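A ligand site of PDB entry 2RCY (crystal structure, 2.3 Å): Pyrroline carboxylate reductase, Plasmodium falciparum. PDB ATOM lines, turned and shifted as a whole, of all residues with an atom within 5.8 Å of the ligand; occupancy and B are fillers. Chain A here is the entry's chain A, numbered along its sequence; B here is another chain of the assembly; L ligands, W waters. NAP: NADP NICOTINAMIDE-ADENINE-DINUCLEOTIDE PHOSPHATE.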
ATOM      1  N   MET A  10      37.101   0.702 -27.942  1.00  0.00           N
ATOM      2  CA  MET A  10      36.589   1.719 -28.854  1.00  0.00           C
ATOM      3  C   MET A  10      35.468   2.503 -28.180  1.00  0.00           C
ATOM      4  O   MET A  10      34.297   2.100 -28.219  1.00  0.00           O
ATOM      5  CB  MET A  10      36.118   1.090 -30.182  1.00  0.00           C
ATOM      6  CG  MET A  10      37.209   0.264 -30.873  1.00  0.00           C
ATOM      7  SD  MET A  10      36.805  -0.240 -32.714  1.00  0.00           S
ATOM      8  CE  MET A  10      35.180  -1.255 -32.421  1.00  0.00           C
ATOM      9  N   GLY A  11      35.845   3.602 -27.541  1.00  0.00           N
ATOM     10  CA  GLY A  11      34.918   4.414 -26.749  1.00  0.00           C
ATOM     11  C   GLY A  11      35.067   4.159 -25.266  1.00  0.00           C
ATOM     12  O   GLY A  11      35.039   3.010 -24.823  1.00  0.00           O
ATOM     13  N   LEU A  12      35.235   5.237 -24.492  1.00  0.00           N
ATOM     14  CA  LEU A  12      35.301   5.143 -23.033  1.00  0.00           C
ATOM     15  C   LEU A  12      34.230   5.990 -22.354  1.00  0.00           C
ATOM     16  O   LEU A  12      34.543   6.952 -21.647  1.00  0.00           O
ATOM     17  CB  LEU A  12      36.697   5.513 -22.508  1.00  0.00           C
ATOM     18  CG  LEU A  12      37.836   4.498 -22.450  1.00  0.00           C
ATOM     19  CD1 LEU A  12      38.847   4.959 -21.428  1.00  0.00           C
ATOM     20  CD2 LEU A  12      37.371   3.093 -22.120  1.00  0.00           C
ATOM     21  N   GLY A  13      32.972   5.621 -22.570  1.00  0.00           N
ATOM     22  CA  GLY A  13      31.849   6.310 -21.941  1.00  0.00           C
ATOM     23  C   GLY A  13      31.633   5.834 -20.528  1.00  0.00           C
ATOM     24  O   GLY A  13      32.586   5.585 -19.791  1.00  0.00           O
ATOM     25  N   GLN A  14      30.367   5.692 -20.141  1.00  0.00           N
ATOM     26  CA  GLN A  14      30.028   5.235 -18.805  1.00  0.00           C
ATOM     27  C   GLN A  14      30.263   3.736 -18.634  1.00  0.00           C
ATOM     28  O   GLN A  14      30.680   3.285 -17.570  1.00  0.00           O
ATOM     29  CB  GLN A  14      28.581   5.599 -18.449  1.00  0.00           C
ATOM     30  CG  GLN A  14      28.337   7.097 -18.254  1.00  0.00           C
ATOM     31  CD  GLN A  14      28.998   7.676 -17.012  1.00  0.00           C
ATOM     32  OE1 GLN A  14      29.473   6.937 -16.139  1.00  0.00           O
ATOM     33  NE2 GLN A  14      29.029   8.999 -16.913  1.00  0.00           N
ATOM     34  N   MET A  15      29.996   2.968 -19.694  1.00  0.00           N
ATOM     35  CA  MET A  15      30.223   1.529 -19.667  1.00  0.00           C
ATOM     36  C   MET A  15      31.652   1.164 -20.065  1.00  0.00           C
ATOM     37  O   MET A  15      32.258   0.264 -19.478  1.00  0.00           O
ATOM     38  CB  MET A  15      29.211   0.792 -20.541  1.00  0.00           C
ATOM     39  CG  MET A  15      29.209  -0.714 -20.341  1.00  0.00           C
ATOM     40  SD  MET A  15      28.789  -1.218 -18.496  1.00  0.00           S
ATOM     41  CE  MET A  15      30.372  -2.284 -18.151  1.00  0.00           C
ATOM     42  N   GLY A  16      32.169   1.864 -21.077  1.00  0.00           N
ATOM     43  CA  GLY A  16      33.527   1.644 -21.558  1.00  0.00           C
ATOM     44  C   GLY A  16      34.577   1.789 -20.469  1.00  0.00           C
ATOM     45  O   GLY A  16      35.429   0.921 -20.301  1.00  0.00           O
ATOM     46  N   TYR A  37      40.354   4.471 -27.645  1.00  0.00           N
ATOM     47  CA  TYR A  37      40.163   5.684 -28.446  1.00  0.00           C
ATOM     48  C   TYR A  37      38.794   6.314 -28.208  1.00  0.00           C
ATOM     49  O   TYR A  37      37.791   5.615 -28.039  1.00  0.00           O
ATOM     50  CB  TYR A  37      40.350   5.415 -29.951  1.00  0.00           C
ATOM     51  CG  TYR A  37      39.879   6.571 -30.822  1.00  0.00           C
ATOM     52  CD1 TYR A  37      40.653   7.715 -30.977  1.00  0.00           C
ATOM     53  CD2 TYR A  37      38.640   6.520 -31.456  1.00  0.00           C
ATOM     54  CE1 TYR A  37      40.219   8.781 -31.767  1.00  0.00           C
ATOM     55  CE2 TYR A  37      38.185   7.577 -32.248  1.00  0.00           C
ATOM     56  CZ  TYR A  37      38.982   8.702 -32.397  1.00  0.00           C
ATOM     57  OH  TYR A  37      38.541   9.749 -33.165  1.00  0.00           O
ATOM     58  N   GLY A  38      38.781   7.640 -28.196  1.00  0.00           N
ATOM     59  CA  GLY A  38      37.557   8.431 -28.174  1.00  0.00           C
ATOM     60  C   GLY A  38      37.791   9.751 -28.890  1.00  0.00           C
ATOM     61  O   GLY A  38      38.949  10.162 -29.047  1.00  0.00           O
ATOM     62  N   PRO A  39      36.708  10.425 -29.314  1.00  0.00           N
ATOM     63  CA  PRO A  39      36.830  11.741 -29.958  1.00  0.00           C
ATOM     64  C   PRO A  39      37.414  12.794 -29.016  1.00  0.00           C
ATOM     65  O   PRO A  39      37.850  13.860 -29.466  1.00  0.00           O
ATOM     66  CB  PRO A  39      35.388  12.093 -30.333  1.00  0.00           C
ATOM     67  CG  PRO A  39      34.545  11.252 -29.442  1.00  0.00           C
ATOM     68  CD  PRO A  39      35.309   9.990 -29.227  1.00  0.00           C
ATOM     69  N   SER A  40      37.398  12.494 -27.715  1.00  0.00           N
ATOM     70  CA  SER A  40      38.026  13.319 -26.700  1.00  0.00           C
ATOM     71  C   SER A  40      38.783  12.429 -25.713  1.00  0.00           C
ATOM     72  O   SER A  40      38.297  11.361 -25.339  1.00  0.00           O
ATOM     73  CB  SER A  40      36.986  14.158 -25.955  1.00  0.00           C
ATOM     74  OG  SER A  40      36.327  15.052 -26.842  1.00  0.00           O
ATOM     75  N   LYS A  42      40.235  10.950 -22.307  1.00  0.00           N
ATOM     76  CA  LYS A  42      39.539  10.712 -21.043  1.00  0.00           C
ATOM     77  C   LYS A  42      40.519  10.620 -19.871  1.00  0.00           C
ATOM     78  O   LYS A  42      41.685  10.285 -20.056  1.00  0.00           O
ATOM     79  CB  LYS A  42      38.713   9.434 -21.137  1.00  0.00           C
ATOM     80  CG  LYS A  42      37.275   9.578 -20.641  1.00  0.00           C
ATOM     81  CD  LYS A  42      36.392  10.214 -21.711  1.00  0.00           C
ATOM     82  CE  LYS A  42      34.960  10.379 -21.219  1.00  0.00           C
ATOM     83  NZ  LYS A  42      34.086  10.970 -22.259  1.00  0.00           N
ATOM     84  N   ASN A  52      40.365   4.404 -34.101  1.00  0.00           N
ATOM     85  CA  ASN A  52      39.833   3.054 -33.960  1.00  0.00           C
ATOM     86  C   ASN A  52      40.518   2.055 -34.886  1.00  0.00           C
ATOM     87  O   ASN A  52      40.678   0.883 -34.533  1.00  0.00           O
ATOM     88  CB  ASN A  52      38.322   3.041 -34.209  1.00  0.00           C
ATOM     89  CG  ASN A  52      37.526   3.702 -33.105  1.00  0.00           C
ATOM     90  OD1 ASN A  52      36.540   4.400 -33.359  1.00  0.00           O
ATOM     91  ND2 ASN A  52      37.934   3.485 -31.857  1.00  0.00           N
ATOM     92  N   CYS A  64      34.006  -3.073 -28.762  1.00  0.00           N
ATOM     93  CA  CYS A  64      33.144  -2.017 -29.288  1.00  0.00           C
ATOM     94  C   CYS A  64      32.272  -1.460 -28.174  1.00  0.00           C
ATOM     95  O   CYS A  64      31.257  -2.066 -27.797  1.00  0.00           O
ATOM     96  CB  CYS A  64      32.295  -2.560 -30.443  1.00  0.00           C
ATOM     97  SG  CYS A  64      31.418  -1.288 -31.374  1.00  0.00           S
ATOM     98  N   ALA A  65      32.674  -0.311 -27.632  1.00  0.00           N
ATOM     99  CA  ALA A  65      32.008   0.282 -26.483  1.00  0.00           C
ATOM    100  C   ALA A  65      31.305   1.601 -26.813  1.00  0.00           C
ATOM    101  O   ALA A  65      31.122   2.459 -25.935  1.00  0.00           O
ATOM    102  CB  ALA A  65      32.999   0.468 -25.336  1.00  0.00           C
ATOM    103  N   VAL A  66      30.917   1.761 -28.070  1.00  0.00           N
ATOM    104  CA  VAL A  66      30.180   2.942 -28.513  1.00  0.00           C
ATOM    105  C   VAL A  66      28.671   2.705 -28.440  1.00  0.00           C
ATOM    106  O   VAL A  66      28.226   1.557 -28.293  1.00  0.00           O
ATOM    107  CB  VAL A  66      30.566   3.376 -29.963  1.00  0.00           C
ATOM    108  CG1 VAL A  66      32.000   3.863 -30.014  1.00  0.00           C
ATOM    109  CG2 VAL A  66      30.336   2.241 -30.958  1.00  0.00           C
ATOM    110  N   LYS A  67      27.893   3.778 -28.533  1.00  0.00           N
ATOM    111  CA  LYS A  67      26.437   3.689 -28.663  1.00  0.00           C
ATOM    112  C   LYS A  67      26.052   2.939 -29.941  1.00  0.00           C
ATOM    113  O   LYS A  67      26.744   3.070 -30.954  1.00  0.00           O
ATOM    114  CB  LYS A  67      25.818   5.096 -28.653  1.00  0.00           C
ATOM    115  CG  LYS A  67      25.706   5.726 -27.261  1.00  0.00           C
ATOM    116  CD  LYS A  67      25.491   7.230 -27.329  1.00  0.00           C
ATOM    117  CE  LYS A  67      24.120   7.600 -27.883  1.00  0.00           C
ATOM    118  NZ  LYS A  67      23.954   9.065 -28.073  1.00  0.00           N
ATOM    119  N   PRO A  68      24.968   2.142 -29.886  1.00  0.00           N
ATOM    120  CA  PRO A  68      24.581   1.273 -31.012  1.00  0.00           C
ATOM    121  C   PRO A  68      24.271   2.008 -32.316  1.00  0.00           C
ATOM    122  O   PRO A  68      24.410   1.420 -33.396  1.00  0.00           O
ATOM    123  CB  PRO A  68      23.336   0.560 -30.487  1.00  0.00           C
ATOM    124  CG  PRO A  68      23.432   0.653 -29.006  1.00  0.00           C
ATOM    125  CD  PRO A  68      24.039   1.997 -28.762  1.00  0.00           C
ATOM    126  N   ILE A  70      25.876   4.604 -33.567  1.00  0.00           N
ATOM    127  CA  ILE A  70      27.129   4.929 -34.260  1.00  0.00           C
ATOM    128  C   ILE A  70      28.073   3.735 -34.396  1.00  0.00           C
ATOM    129  O   ILE A  70      29.176   3.859 -34.938  1.00  0.00           O
ATOM    130  CB  ILE A  70      27.888   6.113 -33.597  1.00  0.00           C
ATOM    131  CG1 ILE A  70      28.070   5.872 -32.093  1.00  0.00           C
ATOM    132  CG2 ILE A  70      27.173   7.434 -33.868  1.00  0.00           C
ATOM    133  CD1 ILE A  70      29.214   6.647 -31.477  1.00  0.00           C
ATOM    134  N   VAL A  74      31.616   2.885 -37.101  1.00  0.00           N
ATOM    135  CA  VAL A  74      32.862   2.568 -36.394  1.00  0.00           C
ATOM    136  C   VAL A  74      33.375   1.170 -36.763  1.00  0.00           C
ATOM    137  O   VAL A  74      34.569   0.988 -37.031  1.00  0.00           O
ATOM    138  CB  VAL A  74      32.691   2.709 -34.846  1.00  0.00           C
ATOM    139  CG1 VAL A  74      33.907   2.158 -34.104  1.00  0.00           C
ATOM    140  CG2 VAL A  74      32.457   4.162 -34.459  1.00  0.00           C
ATOM    141  N   ILE A  90      29.841  -4.911 -26.822  1.00  0.00           N
ATOM    142  CA  ILE A  90      28.996  -4.702 -25.647  1.00  0.00           C
ATOM    143  C   ILE A  90      27.761  -3.864 -25.971  1.00  0.00           C
ATOM    144  O   ILE A  90      27.002  -3.501 -25.067  1.00  0.00           O
ATOM    145  CB  ILE A  90      29.793  -4.096 -24.437  1.00  0.00           C
ATOM    146  CG1 ILE A  90      30.330  -2.700 -24.768  1.00  0.00           C
ATOM    147  CG2 ILE A  90      30.900  -5.040 -23.996  1.00  0.00           C
ATOM    148  CD1 ILE A  90      30.640  -1.851 -23.555  1.00  0.00           C
ATOM    149  N   CYS A  91      27.563  -3.577 -27.250  1.00  0.00           N
ATOM    150  CA  CYS A  91      26.430  -2.787 -27.729  1.00  0.00           C
ATOM    151  C   CYS A  91      25.104  -3.478 -27.450  1.00  0.00           C
ATOM    152  O   CYS A  91      24.933  -4.658 -27.739  1.00  0.00           O
ATOM    153  CB  CYS A  91      26.562  -2.482 -29.223  1.00  0.00           C
ATOM    154  SG  CYS A  91      27.895  -1.349 -29.656  1.00  0.00           S
ATOM    155  N   GLY A  92      24.171  -2.718 -26.874  1.00  0.00           N
ATOM    156  CA  GLY A  92      22.845  -3.222 -26.556  1.00  0.00           C
ATOM    157  C   GLY A  92      21.952  -3.327 -27.778  1.00  0.00           C
ATOM    158  O   GLY A  92      21.914  -2.416 -28.606  1.00  0.00           O
ATOM    159  N   GLY A  93      21.255  -4.452 -27.884  1.00  0.00           N
ATOM    160  CA  GLY A  93      20.329  -4.690 -28.985  1.00  0.00           C
ATOM    161  C   GLY A  93      20.969  -5.333 -30.200  1.00  0.00           C
ATOM    162  O   GLY A  93      20.393  -6.234 -30.810  1.00  0.00           O
ATOM    163  N   MET A 113      27.353  -8.897 -22.810  1.00  0.00           N
ATOM    164  CA  MET A 113      26.519  -7.909 -22.131  1.00  0.00           C
ATOM    165  C   MET A 113      26.957  -7.728 -20.671  1.00  0.00           C
ATOM    166  O   MET A 113      26.689  -8.575 -19.833  1.00  0.00           O
ATOM    167  CB  MET A 113      25.045  -8.283 -22.235  1.00  0.00           C
ATOM    168  CG  MET A 113      24.067  -7.239 -21.702  1.00  0.00           C
ATOM    169  SD  MET A 113      24.392  -5.426 -22.358  1.00  0.00           S
ATOM    170  CE  MET A 113      24.364  -5.757 -24.282  1.00  0.00           C
ATOM    171  N   PRO A 114      27.646  -6.607 -20.382  1.00  0.00           N
ATOM    172  CA  PRO A 114      28.145  -6.277 -19.053  1.00  0.00           C
ATOM    173  C   PRO A 114      27.228  -5.354 -18.248  1.00  0.00           C
ATOM    174  O   PRO A 114      26.169  -4.955 -18.736  1.00  0.00           O
ATOM    175  CB  PRO A 114      29.449  -5.543 -19.361  1.00  0.00           C
ATOM    176  CG  PRO A 114      29.187  -4.851 -20.684  1.00  0.00           C
ATOM    177  CD  PRO A 114      28.045  -5.580 -21.368  1.00  0.00           C
ATOM    178  N   ASN A 115      27.632  -5.058 -17.025  1.00  0.00           N
ATOM    179  CA  ASN A 115      27.029  -3.970 -16.247  1.00  0.00           C
ATOM    180  C   ASN A 115      28.094  -3.167 -15.480  1.00  0.00           C
ATOM    181  O   ASN A 115      29.223  -3.639 -15.320  1.00  0.00           O
ATOM    182  CB  ASN A 115      25.909  -4.468 -15.328  1.00  0.00           C
ATOM    183  CG  ASN A 115      26.367  -5.523 -14.323  1.00  0.00           C
ATOM    184  OD1 ASN A 115      27.559  -5.687 -14.075  1.00  0.00           O
ATOM    185  ND2 ASN A 115      25.408  -6.224 -13.731  1.00  0.00           N
ATOM    186  N   THR A 116      27.743  -1.965 -15.033  1.00  0.00           N
ATOM    187  CA  THR A 116      28.693  -1.050 -14.388  1.00  0.00           C
ATOM    188  C   THR A 116      29.383  -1.569 -13.102  1.00  0.00           C
ATOM    189  O   THR A 116      30.531  -1.195 -12.847  1.00  0.00           O
ATOM    190  CB  THR A 116      28.095   0.360 -14.122  1.00  0.00           C
ATOM    191  OG1 THR A 116      26.907   0.251 -13.335  1.00  0.00           O
ATOM    192  CG2 THR A 116      27.781   1.071 -15.432  1.00  0.00           C
ATOM    193  N   GLY A 167      22.140  -6.365 -17.536  1.00  0.00           N
ATOM    194  CA  GLY A 167      22.655  -5.097 -18.063  1.00  0.00           C
ATOM    195  C   GLY A 167      21.965  -3.886 -17.487  1.00  0.00           C
ATOM    196  O   GLY A 167      22.622  -2.959 -17.016  1.00  0.00           O
ATOM    197  N   ASN B 222      24.337   6.804 -14.834  1.00  0.00           N
ATOM    198  CA  ASN B 222      25.478   6.260 -15.587  1.00  0.00           C
ATOM    199  C   ASN B 222      25.129   5.066 -16.452  1.00  0.00           C
ATOM    200  O   ASN B 222      25.773   4.804 -17.465  1.00  0.00           O
ATOM    201  CB  ASN B 222      26.616   5.898 -14.630  1.00  0.00           C
ATOM    202  CG  ASN B 222      27.205   7.100 -13.916  1.00  0.00           C
ATOM    203  OD1 ASN B 222      27.168   8.232 -14.424  1.00  0.00           O
ATOM    204  ND2 ASN B 222      27.746   6.883 -12.726  1.00  0.00           N
ATOM    205  N   ILE B 223      24.095   4.334 -16.046  1.00  0.00           N
ATOM    206  CA  ILE B 223      23.656   3.136 -16.766  1.00  0.00           C
ATOM    207  C   ILE B 223      22.671   3.460 -17.886  1.00  0.00           C
ATOM    208  O   ILE B 223      22.380   2.624 -18.743  1.00  0.00           O
ATOM    209  CB  ILE B 223      23.118   2.058 -15.764  1.00  0.00           C
ATOM    210  CG1 ILE B 223      22.390   0.920 -16.503  1.00  0.00           C
ATOM    211  CG2 ILE B 223      22.222   2.682 -14.704  1.00  0.00           C
ATOM    212  CD1 ILE B 223      21.934  -0.183 -15.601  1.00  0.00           C
ATOM    213  N   VAL B 224      22.171   4.697 -17.907  1.00  0.00           N
ATOM    214  CA  VAL B 224      21.239   5.129 -18.927  1.00  0.00           C
ATOM    215  C   VAL B 224      21.982   5.660 -20.144  1.00  0.00           C
ATOM    216  O   VAL B 224      22.352   6.839 -20.201  1.00  0.00           O
ATOM    217  CB  VAL B 224      20.232   6.184 -18.398  1.00  0.00           C
ATOM    218  CG1 VAL B 224      19.106   6.389 -19.390  1.00  0.00           C
ATOM    219  CG2 VAL B 224      19.662   5.753 -17.059  1.00  0.00           C
ATOM    220  N   SER B 225      22.218   4.776 -21.114  1.00  0.00           N
ATOM    221  CA  SER B 225      22.800   5.162 -22.383  1.00  0.00           C
ATOM    222  C   SER B 225      21.733   5.869 -23.208  1.00  0.00           C
ATOM    223  O   SER B 225      20.620   5.343 -23.363  1.00  0.00           O
ATOM    224  CB  SER B 225      23.308   3.932 -23.147  1.00  0.00           C
ATOM    225  OG  SER B 225      24.149   3.141 -22.331  1.00  0.00           O
ATOM    226  N   PRO B 226      22.044   7.089 -23.706  1.00  0.00           N
ATOM    227  CA  PRO B 226      21.109   7.883 -24.502  1.00  0.00           C
ATOM    228  C   PRO B 226      20.453   7.086 -25.636  1.00  0.00           C
ATOM    229  O   PRO B 226      21.155   6.500 -26.467  1.00  0.00           O
ATOM    230  CB  PRO B 226      21.991   8.995 -25.057  1.00  0.00           C
ATOM    231  CG  PRO B 226      23.042   9.174 -24.015  1.00  0.00           C
ATOM    232  CD  PRO B 226      23.330   7.788 -23.511  1.00  0.00           C
ATOM    233  N   ILE B 229      18.301   0.959 -23.903  1.00  0.00           N
ATOM    234  CA  ILE B 229      17.388  -0.049 -23.358  1.00  0.00           C
ATOM    235  C   ILE B 229      16.953   0.268 -21.916  1.00  0.00           C
ATOM    236  O   ILE B 229      15.766   0.172 -21.590  1.00  0.00           O
ATOM    237  CB  ILE B 229      18.040  -1.461 -23.414  1.00  0.00           C
ATOM    238  CG1 ILE B 229      18.482  -1.783 -24.845  1.00  0.00           C
ATOM    239  CG2 ILE B 229      17.091  -2.530 -22.872  1.00  0.00           C
ATOM    240  CD1 ILE B 229      19.488  -2.908 -24.945  1.00  0.00           C
ATOM    241  N   THR B 230      17.909   0.642 -21.078  1.00  0.00           N
ATOM    242  CA  THR B 230      17.677   0.942 -19.664  1.00  0.00           C
ATOM    243  C   THR B 230      16.685   2.087 -19.495  1.00  0.00           C
ATOM    244  O   THR B 230      15.819   2.040 -18.626  1.00  0.00           O
ATOM    245  CB  THR B 230      19.005   1.268 -18.945  1.00  0.00           C
ATOM    246  OG1 THR B 230      19.912   0.170 -19.089  1.00  0.00           O
ATOM    247  CG2 THR B 230      18.777   1.529 -17.462  1.00  0.00           C
HETATM  248  PA  NAP L   1      28.160   6.775 -23.525  1.00  0.00           P
HETATM  249  O1A NAP L   1      28.477   7.124 -22.085  1.00  0.00           O
HETATM  250  O2A NAP L   1      27.521   7.823 -24.405  1.00  0.00           O
HETATM  251  O5B NAP L   1      29.509   6.230 -24.217  1.00  0.00           O
HETATM  252  C5B NAP L   1      29.812   6.438 -25.597  1.00  0.00           C
HETATM  253  C4B NAP L   1      31.259   6.898 -25.693  1.00  0.00           C
HETATM  254  O4B NAP L   1      31.783   6.648 -26.994  1.00  0.00           O
HETATM  255  C3B NAP L   1      31.387   8.401 -25.431  1.00  0.00           C
HETATM  256  O3B NAP L   1      32.220   8.601 -24.292  1.00  0.00           O
HETATM  257  C2B NAP L   1      32.021   8.981 -26.687  1.00  0.00           C
HETATM  258  O2B NAP L   1      33.062   9.898 -26.369  1.00  0.00           O
HETATM  259  C1B NAP L   1      32.575   7.768 -27.418  1.00  0.00           C
HETATM  260  N9A NAP L   1      32.516   7.893 -28.901  1.00  0.00           N
HETATM  261  C8A NAP L   1      31.657   8.642 -29.620  1.00  0.00           C
HETATM  262  N7A NAP L   1      31.931   8.486 -30.932  1.00  0.00           N
HETATM  263  C5A NAP L   1      32.956   7.620 -31.043  1.00  0.00           C
HETATM  264  C6A NAP L   1      33.660   7.079 -32.115  1.00  0.00           C
HETATM  265  N6A NAP L   1      33.328   7.414 -33.386  1.00  0.00           N
HETATM  266  N1A NAP L   1      34.670   6.214 -31.881  1.00  0.00           N
HETATM  267  C2A NAP L   1      35.011   5.869 -30.629  1.00  0.00           C
HETATM  268  N3A NAP L   1      34.347   6.376 -29.567  1.00  0.00           N
HETATM  269  C4A NAP L   1      33.318   7.247 -29.753  1.00  0.00           C
HETATM  270  O3  NAP L   1      27.238   5.466 -23.552  1.00  0.00           O
HETATM  271  PN  NAP L   1      27.521   4.200 -22.600  1.00  0.00           P
HETATM  272  O1N NAP L   1      26.488   4.208 -21.502  1.00  0.00           O
HETATM  273  O2N NAP L   1      28.991   4.164 -22.244  1.00  0.00           O
HETATM  274  O5D NAP L   1      27.184   2.949 -23.546  1.00  0.00           O
HETATM  275  C5D NAP L   1      28.045   2.526 -24.592  1.00  0.00           C
HETATM  276  C4D NAP L   1      27.631   1.133 -25.043  1.00  0.00           C
HETATM  277  O4D NAP L   1      27.682   0.221 -23.939  1.00  0.00           O
HETATM  278  C3D NAP L   1      26.203   1.105 -25.577  1.00  0.00           C
HETATM  279  O3D NAP L   1      26.208   0.444 -26.852  1.00  0.00           O
HETATM  280  C2D NAP L   1      25.403   0.303 -24.566  1.00  0.00           C
HETATM  281  O2D NAP L   1      24.431  -0.552 -25.182  1.00  0.00           O
HETATM  282  C1D NAP L   1      26.461  -0.523 -23.844  1.00  0.00           C
HETATM  283  N1N NAP L   1      26.122  -0.803 -22.446  1.00  0.00           N
HETATM  284  C2N NAP L   1      26.030   0.190 -21.541  1.00  0.00           C
HETATM  285  C3N NAP L   1      25.711  -0.088 -20.222  1.00  0.00           C
HETATM  286  C7N NAP L   1      25.629   1.024 -19.214  1.00  0.00           C
HETATM  287  O7N NAP L   1      25.782   2.295 -19.593  1.00  0.00           O
HETATM  288  N7N NAP L   1      25.425   0.757 -18.008  1.00  0.00           N
HETATM  289  C4N NAP L   1      25.489  -1.404 -19.822  1.00  0.00           C
HETATM  290  C5N NAP L   1      25.593  -2.412 -20.774  1.00  0.00           C
HETATM  291  C6N NAP L   1      25.914  -2.083 -22.091  1.00  0.00           C
HETATM  292  P2B NAP L   1      32.764  11.442 -26.004  1.00  0.00           P
HETATM  293  O1X NAP L   1      34.110  12.114 -26.155  1.00  0.00           O
HETATM  294  O2X NAP L   1      31.730  11.896 -27.017  1.00  0.00           O
HETATM  295  O3X NAP L   1      32.264  11.406 -24.581  1.00  0.00           O
HETATM  296  O   HOH W   1      24.840  -1.594 -16.361  1.00  0.00           O
HETATM  297  O   HOH W   2      29.935   9.901 -21.363  1.00  0.00           O
HETATM  298  O   HOH W   3      21.599   0.657 -25.165  1.00  0.00           O
HETATM  299  O   HOH W   4      25.571   5.998 -19.894  1.00  0.00           O
HETATM  300  O   HOH W   5      31.562   3.487 -23.587  1.00  0.00           O
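An oxygen (O7N) of the ligand sits close to the backbone carbonyl oxygen (O) of Asn 222 of chain B, 3.3 Å away.
CA of Gly 11 touches N3A of the ligand, 3.5 Å away.
C of Leu 12 touches O3B of the ligand, 3.8 Å away.
Gly 13 touches the ligand (CA to O5B, 3.3 Å).
Tyr 37 touches the ligand (CD2 to C2A, 3.8 Å).
CG of Pro 39 touches O1X of the ligand, at 3.4 Å.
Ser 40 touches the ligand.
Ala 65 touches the ligand (O to C5D, 3.4 Å).
Lys 67 touches the ligand (CD to O2A, 3.6 Å).
Pro 68 touches the ligand (CD to O3D, 3.3 Å).
CD1 of Ile 70 touches N7A of the ligand, 3.3 Å away.
Val 74 touches the ligand.
Ile 90 touches the ligand (O to C1D, 3.3 Å).
Met 113 touches the ligand (SD to C5N, 3.6 Å).
Pro 114 touches the ligand.
CG2 of Thr 116 touches N7N of the ligand, at 3.5 Å.
CA of Ile 223 of chain B touches N7N of the ligand (3.2 Å).
Hydrophobic or aromatic side chains within 4 Å of the ligand: Met 15, Tyr 37, Pro 39, Val 66, Pro 68, Ile 70, Val 74, Ile 90, Met 113 and Ile 223 of chain B.
Of the 36 residues printed, 25 come within 4 Å of the ligand.
The nearest printed residue that does not touch the ligand is Gly 38 (4.1 Å).
An oxygen (O1N) of the ligand lies within hydrogen-bond range of the side-chain hydroxyl (OG) of Ser 225 of chain B.
The backbone carbonyl oxygen of Val 66 lies within hydrogen-bond range of an oxygen (O3D) of the ligand, 2.7 Å away.
The backbone NH (N) of Gly 92 is in hydrogen-bond range of an oxygen (O2D) of the ligand (2.8 Å).
The backbone NH (N) of Gln 14 lies within hydrogen-bond range of an oxygen (O2N) of the ligand (2.9 Å).
The side-chain amino group (NZ) of Lys 42 is in salt-bridge range of an oxygen (O3X) of the ligand.
N of Met 15 lies within hydrogen-bond range of O2N of the ligand.
The side-chain amide oxygen (OD1) of Asn 52 sits close to a nitrogen (N1A) of the ligand, 3.0 Å away.
O3D of the ligand lies close to SG of Cys 91 (3.7 Å).
The side-chain sulfur (SG) of Cys 91 is in hydrogen-bond range of the backbone carbonyl oxygen (O) of Val 66 (3.2 Å).
O of Met 10 sits at hydrogen-bond distance from N of Val 66.
The side-chain amide oxygen (OD1) of Asn 222 of chain B lies close to the side-chain amide oxygen (OE1) of Gln 14, 3.2 Å away.
SD of Met 15 is in hydrogen-bond range of N of Thr 116.
OG1 of Thr 230 of chain B sits at hydrogen-bond distance from O of Ile 223 of chain B (3.5 Å).
The backbone NH of Ile 90 sits close to the backbone carbonyl oxygen of Cys 64.
N of Ala 65 lies within hydrogen-bond range of O of Met 10 (3.0 Å).
The backbone NH (N) of Gly 11 is in hydrogen-bond range of the backbone carbonyl oxygen (O) of Tyr 37, 2.8 Å away.
Water W4 lies within hydrogen-bond range of O1N of the ligand (2.6 Å), O of Asn 222 of chain B (2.7 Å) and O of Val 224 of chain B (3.3 Å).
Water W1 lies within hydrogen-bond range of the backbone carbonyl oxygen of Gly 167, a nitrogen (N7N) of the ligand and the backbone NH of Thr 116.
Water W5 lies within hydrogen-bond range of the backbone carbonyl oxygen (O) of Ala 65, the backbone NH (N) of Gly 13, an oxygen (O2N) of the ligand and the backbone NH (N) of Gly 16.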
